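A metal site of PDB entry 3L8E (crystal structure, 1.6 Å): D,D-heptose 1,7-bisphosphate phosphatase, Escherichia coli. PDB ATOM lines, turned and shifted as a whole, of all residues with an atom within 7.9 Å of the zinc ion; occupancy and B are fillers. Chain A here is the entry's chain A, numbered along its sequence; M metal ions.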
ATOM      1  N   THR A  53     -24.701 -17.904 -20.502  1.00  0.00           N
ATOM      2  CA  THR A  53     -23.577 -17.498 -19.658  1.00  0.00           C
ATOM      3  C   THR A  53     -23.213 -16.016 -19.766  1.00  0.00           C
ATOM      4  O   THR A  53     -23.020 -15.487 -20.852  1.00  0.00           O
ATOM      5  CB  THR A  53     -22.331 -18.406 -19.924  1.00  0.00           C
ATOM      6  OG1 THR A  53     -21.257 -18.035 -19.072  1.00  0.00           O
ATOM      7  CG2 THR A  53     -21.856 -18.339 -21.372  1.00  0.00           C
ATOM      8  N   ASN A  54     -23.109 -15.371 -18.601  1.00  0.00           N
ATOM      9  CA  ASN A  54     -22.536 -14.025 -18.542  1.00  0.00           C
ATOM     10  C   ASN A  54     -21.016 -14.163 -18.642  1.00  0.00           C
ATOM     11  O   ASN A  54     -20.417 -14.933 -17.883  1.00  0.00           O
ATOM     12  CB  ASN A  54     -22.883 -13.329 -17.209  1.00  0.00           C
ATOM     13  CG  ASN A  54     -24.263 -12.667 -17.202  1.00  0.00           C
ATOM     14  OD1 ASN A  54     -25.036 -12.708 -18.176  1.00  0.00           O
ATOM     15  ND2 ASN A  54     -24.581 -12.039 -16.072  1.00  0.00           N
ATOM     16  N   GLN A  55     -20.404 -13.444 -19.576  1.00  0.00           N
ATOM     17  CA  GLN A  55     -18.960 -13.485 -19.779  1.00  0.00           C
ATOM     18  C   GLN A  55     -18.420 -12.061 -19.798  1.00  0.00           C
ATOM     19  O   GLN A  55     -17.912 -11.587 -20.823  1.00  0.00           O
ATOM     20  CB  GLN A  55     -18.611 -14.214 -21.078  1.00  0.00           C
ATOM     21  CG  GLN A  55     -18.905 -15.733 -21.049  1.00  0.00           C
ATOM     22  CD  GLN A  55     -17.975 -16.479 -20.098  1.00  0.00           C
ATOM     23  OE1 GLN A  55     -16.784 -16.181 -20.025  1.00  0.00           O
ATOM     24  NE2 GLN A  55     -18.504 -17.459 -19.376  1.00  0.00           N
ATOM     25  N   TYR A  91     -24.349 -16.432 -24.863  1.00  0.00           N
ATOM     26  CA  TYR A  91     -23.496 -15.714 -23.934  1.00  0.00           C
ATOM     27  C   TYR A  91     -23.726 -14.218 -24.016  1.00  0.00           C
ATOM     28  O   TYR A  91     -24.218 -13.711 -25.032  1.00  0.00           O
ATOM     29  CB  TYR A  91     -22.027 -16.024 -24.211  1.00  0.00           C
ATOM     30  CG  TYR A  91     -21.511 -15.468 -25.503  1.00  0.00           C
ATOM     31  CD1 TYR A  91     -21.811 -16.103 -26.704  1.00  0.00           C
ATOM     32  CD2 TYR A  91     -20.708 -14.332 -25.540  1.00  0.00           C
ATOM     33  CE1 TYR A  91     -21.331 -15.617 -27.901  1.00  0.00           C
ATOM     34  CE2 TYR A  91     -20.207 -13.841 -26.741  1.00  0.00           C
ATOM     35  CZ  TYR A  91     -20.526 -14.488 -27.914  1.00  0.00           C
ATOM     36  OH  TYR A  91     -20.056 -14.015 -29.127  1.00  0.00           O
ATOM     37  N   CYS A  92     -23.372 -13.531 -22.937  1.00  0.00           N
ATOM     38  CA  CYS A  92     -23.375 -12.069 -22.924  1.00  0.00           C
ATOM     39  C   CYS A  92     -21.969 -11.578 -22.613  1.00  0.00           C
ATOM     40  O   CYS A  92     -21.432 -11.832 -21.525  1.00  0.00           O
ATOM     41  CB  CYS A  92     -24.337 -11.561 -21.863  1.00  0.00           C
ATOM     42  SG  CYS A  92     -24.095  -9.803 -21.557  1.00  0.00           S
ATOM     43  N   PRO A  93     -21.347 -10.887 -23.581  1.00  0.00           N
ATOM     44  CA  PRO A  93     -19.994 -10.353 -23.398  1.00  0.00           C
ATOM     45  C   PRO A  93     -19.989  -8.937 -22.821  1.00  0.00           C
ATOM     46  O   PRO A  93     -18.914  -8.373 -22.664  1.00  0.00           O
ATOM     47  CB  PRO A  93     -19.461 -10.294 -24.828  1.00  0.00           C
ATOM     48  CG  PRO A  93     -20.697  -9.930 -25.615  1.00  0.00           C
ATOM     49  CD  PRO A  93     -21.834 -10.687 -24.955  1.00  0.00           C
ATOM     50  N   HIS A  94     -21.162  -8.382 -22.528  1.00  0.00           N
ATOM     51  CA  HIS A  94     -21.276  -6.957 -22.232  1.00  0.00           C
ATOM     52  C   HIS A  94     -21.099  -6.606 -20.762  1.00  0.00           C
ATOM     53  O   HIS A  94     -21.293  -7.422 -19.879  1.00  0.00           O
ATOM     54  CB  HIS A  94     -22.652  -6.428 -22.679  1.00  0.00           C
ATOM     55  CG  HIS A  94     -22.973  -6.726 -24.110  1.00  0.00           C
ATOM     56  ND1 HIS A  94     -23.979  -7.581 -24.478  1.00  0.00           N
ATOM     57  CD2 HIS A  94     -22.405  -6.283 -25.258  1.00  0.00           C
ATOM     58  CE1 HIS A  94     -24.025  -7.644 -25.801  1.00  0.00           C
ATOM     59  NE2 HIS A  94     -23.086  -6.869 -26.297  1.00  0.00           N
ATOM     60  N   HIS A  95     -20.762  -5.337 -20.530  1.00  0.00           N
ATOM     61  CA  HIS A  95     -20.809  -4.743 -19.203  1.00  0.00           C
ATOM     62  C   HIS A  95     -20.900  -3.238 -19.399  1.00  0.00           C
ATOM     63  O   HIS A  95     -20.205  -2.677 -20.208  1.00  0.00           O
ATOM     64  CB  HIS A  95     -19.557  -5.078 -18.418  1.00  0.00           C
ATOM     65  CG  HIS A  95     -19.667  -4.785 -16.949  1.00  0.00           C
ATOM     66  ND1 HIS A  95     -19.596  -3.520 -16.431  1.00  0.00           N
ATOM     67  CD2 HIS A  95     -19.847  -5.616 -15.902  1.00  0.00           C
ATOM     68  CE1 HIS A  95     -19.727  -3.567 -15.123  1.00  0.00           C
ATOM     69  NE2 HIS A  95     -19.874  -4.836 -14.763  1.00  0.00           N
ATOM     70  N   PHE A 103     -17.883  -3.671 -26.327  1.00  0.00           N
ATOM     71  CA  PHE A 103     -18.756  -4.431 -25.425  1.00  0.00           C
ATOM     72  C   PHE A 103     -19.256  -3.588 -24.270  1.00  0.00           C
ATOM     73  O   PHE A 103     -19.947  -4.078 -23.371  1.00  0.00           O
ATOM     74  CB  PHE A 103     -18.038  -5.687 -24.937  1.00  0.00           C
ATOM     75  CG  PHE A 103     -17.565  -6.548 -26.061  1.00  0.00           C
ATOM     76  CD1 PHE A 103     -18.452  -7.321 -26.794  1.00  0.00           C
ATOM     77  CD2 PHE A 103     -16.219  -6.568 -26.412  1.00  0.00           C
ATOM     78  CE1 PHE A 103     -18.019  -8.102 -27.847  1.00  0.00           C
ATOM     79  CE2 PHE A 103     -15.786  -7.348 -27.465  1.00  0.00           C
ATOM     80  CZ  PHE A 103     -16.693  -8.111 -28.189  1.00  0.00           C
ATOM     81  N   GLN A 105     -21.673  -1.476 -22.740  1.00  0.00           N
ATOM     82  CA  GLN A 105     -23.045  -1.075 -22.926  1.00  0.00           C
ATOM     83  C   GLN A 105     -23.925  -1.755 -21.914  1.00  0.00           C
ATOM     84  O   GLN A 105     -23.577  -2.806 -21.366  1.00  0.00           O
ATOM     85  CB  GLN A 105     -23.530  -1.473 -24.324  1.00  0.00           C
ATOM     86  CG  GLN A 105     -23.631  -2.974 -24.526  1.00  0.00           C
ATOM     87  CD  GLN A 105     -24.294  -3.347 -25.861  1.00  0.00           C
ATOM     88  OE1 GLN A 105     -25.509  -3.511 -25.938  1.00  0.00           O
ATOM     89  NE2 GLN A 105     -23.485  -3.482 -26.894  1.00  0.00           N
ATOM     90  N   VAL A 106     -25.081  -1.142 -21.687  1.00  0.00           N
ATOM     91  CA  VAL A 106     -26.213  -1.814 -21.101  1.00  0.00           C
ATOM     92  C   VAL A 106     -26.824  -2.691 -22.189  1.00  0.00           C
ATOM     93  O   VAL A 106     -26.756  -2.359 -23.382  1.00  0.00           O
ATOM     94  CB  VAL A 106     -27.247  -0.786 -20.591  1.00  0.00           C
ATOM     95  CG1 VAL A 106     -28.592  -1.452 -20.317  1.00  0.00           C
ATOM     96  CG2 VAL A 106     -26.721  -0.095 -19.338  1.00  0.00           C
ATOM     97  N   CYS A 107     -27.389  -3.822 -21.793  1.00  0.00           N
ATOM     98  CA  CYS A 107     -27.950  -4.750 -22.771  1.00  0.00           C
ATOM     99  C   CYS A 107     -29.125  -5.544 -22.211  1.00  0.00           C
ATOM    100  O   CYS A 107     -29.467  -5.418 -21.031  1.00  0.00           O
ATOM    101  CB  CYS A 107     -26.875  -5.702 -23.260  1.00  0.00           C
ATOM    102  SG  CYS A 107     -26.299  -6.831 -21.968  1.00  0.00           S
ATOM    103  N   ASP A 108     -29.741  -6.350 -23.068  1.00  0.00           N
ATOM    104  CA  ASP A 108     -30.866  -7.172 -22.641  1.00  0.00           C
ATOM    105  C   ASP A 108     -30.420  -8.591 -22.332  1.00  0.00           C
ATOM    106  O   ASP A 108     -31.216  -9.391 -21.820  1.00  0.00           O
ATOM    107  CB  ASP A 108     -31.966  -7.192 -23.707  1.00  0.00           C
ATOM    108  CG  ASP A 108     -32.796  -5.922 -23.716  1.00  0.00           C
ATOM    109  OD1 ASP A 108     -33.072  -5.376 -22.625  1.00  0.00           O
ATOM    110  OD2 ASP A 108     -33.177  -5.484 -24.815  1.00  0.00           O
ATOM    111  N   CYS A 109     -29.166  -8.907 -22.627  1.00  0.00           N
ATOM    112  CA  CYS A 109     -28.710 -10.283 -22.463  1.00  0.00           C
ATOM    113  C   CYS A 109     -27.908 -10.537 -21.188  1.00  0.00           C
ATOM    114  O   CYS A 109     -27.653 -11.692 -20.839  1.00  0.00           O
ATOM    115  CB  CYS A 109     -27.949 -10.796 -23.704  1.00  0.00           C
ATOM    116  SG  CYS A 109     -26.809  -9.625 -24.509  1.00  0.00           S
ATOM    117  N   ARG A 110     -27.509  -9.485 -20.486  1.00  0.00           N
ATOM    118  CA  ARG A 110     -26.772  -9.684 -19.246  1.00  0.00           C
ATOM    119  C   ARG A 110     -27.711 -10.013 -18.102  1.00  0.00           C
ATOM    120  O   ARG A 110     -28.504  -9.153 -17.673  1.00  0.00           O
ATOM    121  CB  ARG A 110     -25.908  -8.470 -18.890  1.00  0.00           C
ATOM    122  CG  ARG A 110     -25.093  -8.635 -17.596  1.00  0.00           C
ATOM    123  CD  ARG A 110     -23.968  -7.603 -17.500  1.00  0.00           C
ATOM    124  NE  ARG A 110     -23.390  -7.560 -16.162  1.00  0.00           N
ATOM    125  CZ  ARG A 110     -22.438  -8.390 -15.718  1.00  0.00           C
ATOM    126  NH1 ARG A 110     -21.937  -9.335 -16.503  1.00  0.00           N
ATOM    127  NH2 ARG A 110     -21.992  -8.260 -14.474  1.00  0.00           N
ATOM    128  N   LYS A 111     -27.646 -11.251 -17.615  1.00  0.00           N
ATOM    129  CA  LYS A 111     -28.428 -11.628 -16.437  1.00  0.00           C
ATOM    130  C   LYS A 111     -28.087 -10.616 -15.338  1.00  0.00           C
ATOM    131  O   LYS A 111     -26.933 -10.268 -15.151  1.00  0.00           O
ATOM    132  CB  LYS A 111     -28.106 -13.067 -15.999  1.00  0.00           C
ATOM    133  CG  LYS A 111     -28.399 -14.104 -17.105  1.00  0.00           C
ATOM    134  CD  LYS A 111     -27.918 -15.501 -16.732  1.00  0.00           C
ATOM    135  CE  LYS A 111     -26.399 -15.570 -16.729  1.00  0.00           C
ATOM    136  NZ  LYS A 111     -25.932 -16.935 -16.292  1.00  0.00           N
ATOM    137  N   HIS A 113     -31.087  -9.603 -16.661  1.00  0.00           N
ATOM    138  CA  HIS A 113     -31.982  -9.439 -17.817  1.00  0.00           C
ATOM    139  C   HIS A 113     -32.177 -10.843 -18.388  1.00  0.00           C
ATOM    140  O   HIS A 113     -31.231 -11.628 -18.411  1.00  0.00           O
ATOM    141  CB  HIS A 113     -31.347  -8.547 -18.893  1.00  0.00           C
ATOM    142  CG  HIS A 113     -31.086  -7.141 -18.458  1.00  0.00           C
ATOM    143  ND1 HIS A 113     -29.844  -6.701 -18.046  1.00  0.00           N
ATOM    144  CD2 HIS A 113     -31.891  -6.051 -18.424  1.00  0.00           C
ATOM    145  CE1 HIS A 113     -29.900  -5.422 -17.755  1.00  0.00           C
ATOM    146  NE2 HIS A 113     -31.139  -4.998 -17.974  1.00  0.00           N
ATOM    147  N   MET A 116     -31.101 -13.781 -22.943  1.00  0.00           N
ATOM    148  CA  MET A 116     -30.574 -15.049 -23.459  1.00  0.00           C
ATOM    149  C   MET A 116     -31.606 -16.168 -23.362  1.00  0.00           C
ATOM    150  O   MET A 116     -31.708 -17.025 -24.243  1.00  0.00           O
ATOM    151  CB  MET A 116     -29.301 -15.459 -22.713  1.00  0.00           C
ATOM    152  CG  MET A 116     -28.098 -14.594 -23.003  1.00  0.00           C
ATOM    153  SD  MET A 116     -26.572 -15.244 -22.269  1.00  0.00           S
ATOM    154  CE  MET A 116     -26.774 -14.883 -20.516  1.00  0.00           C
HETATM  155 ZN    ZN M   1     -25.304  -8.627 -23.100  1.00  0.00          ZN
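The backbone NH (N) of Arg 110 lies close to the side-chain sulfur (SG) of Cys 107 (3.3 Å).
The backbone NH of Gln 55 sits at hydrogen-bond distance from the backbone carbonyl oxygen of Cys 92, at 2.7 Å.
The side-chain amide nitrogen (NE2) of Gln 105 sits close to a ring nitrogen (NE2) of His 94 (3.5 Å).
The backbone carbonyl oxygen of Cys 107 lies within hydrogen-bond range of a ring nitrogen (ND1) of His 113 (3.3 Å).
N of Cys 92 is in hydrogen-bond range of SD of Met 116 (3.7 Å).
A ring nitrogen (ND1) of His 113 lies within hydrogen-bond range of the backbone carbonyl oxygen (O) of Arg 110, 2.8 Å away.
The backbone NH (N) of Cys 92 sits at hydrogen-bond distance from the backbone carbonyl oxygen (O) of Thr 53 (2.9 Å).
The side-chain sulfur (SG) of Cys 92 lies close to the backbone NH (N) of Arg 110 (3.6 Å).
Residues that only touch the zinc ion: Arg 110 (3.5 Å).
The nearest printed residue that does not touch the zinc ion is Pro 93 (4.4 Å).
The zinc ion is bound by a ring nitrogen (ND1) of His 94.
The side-chain sulfur (SG) of Cys 92 binds the zinc ion, at 2.3 Å.
SG of Cys 109 is bound to the zinc ion (2.3 Å).
SG of Cys 107 is bound to the zinc ion.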
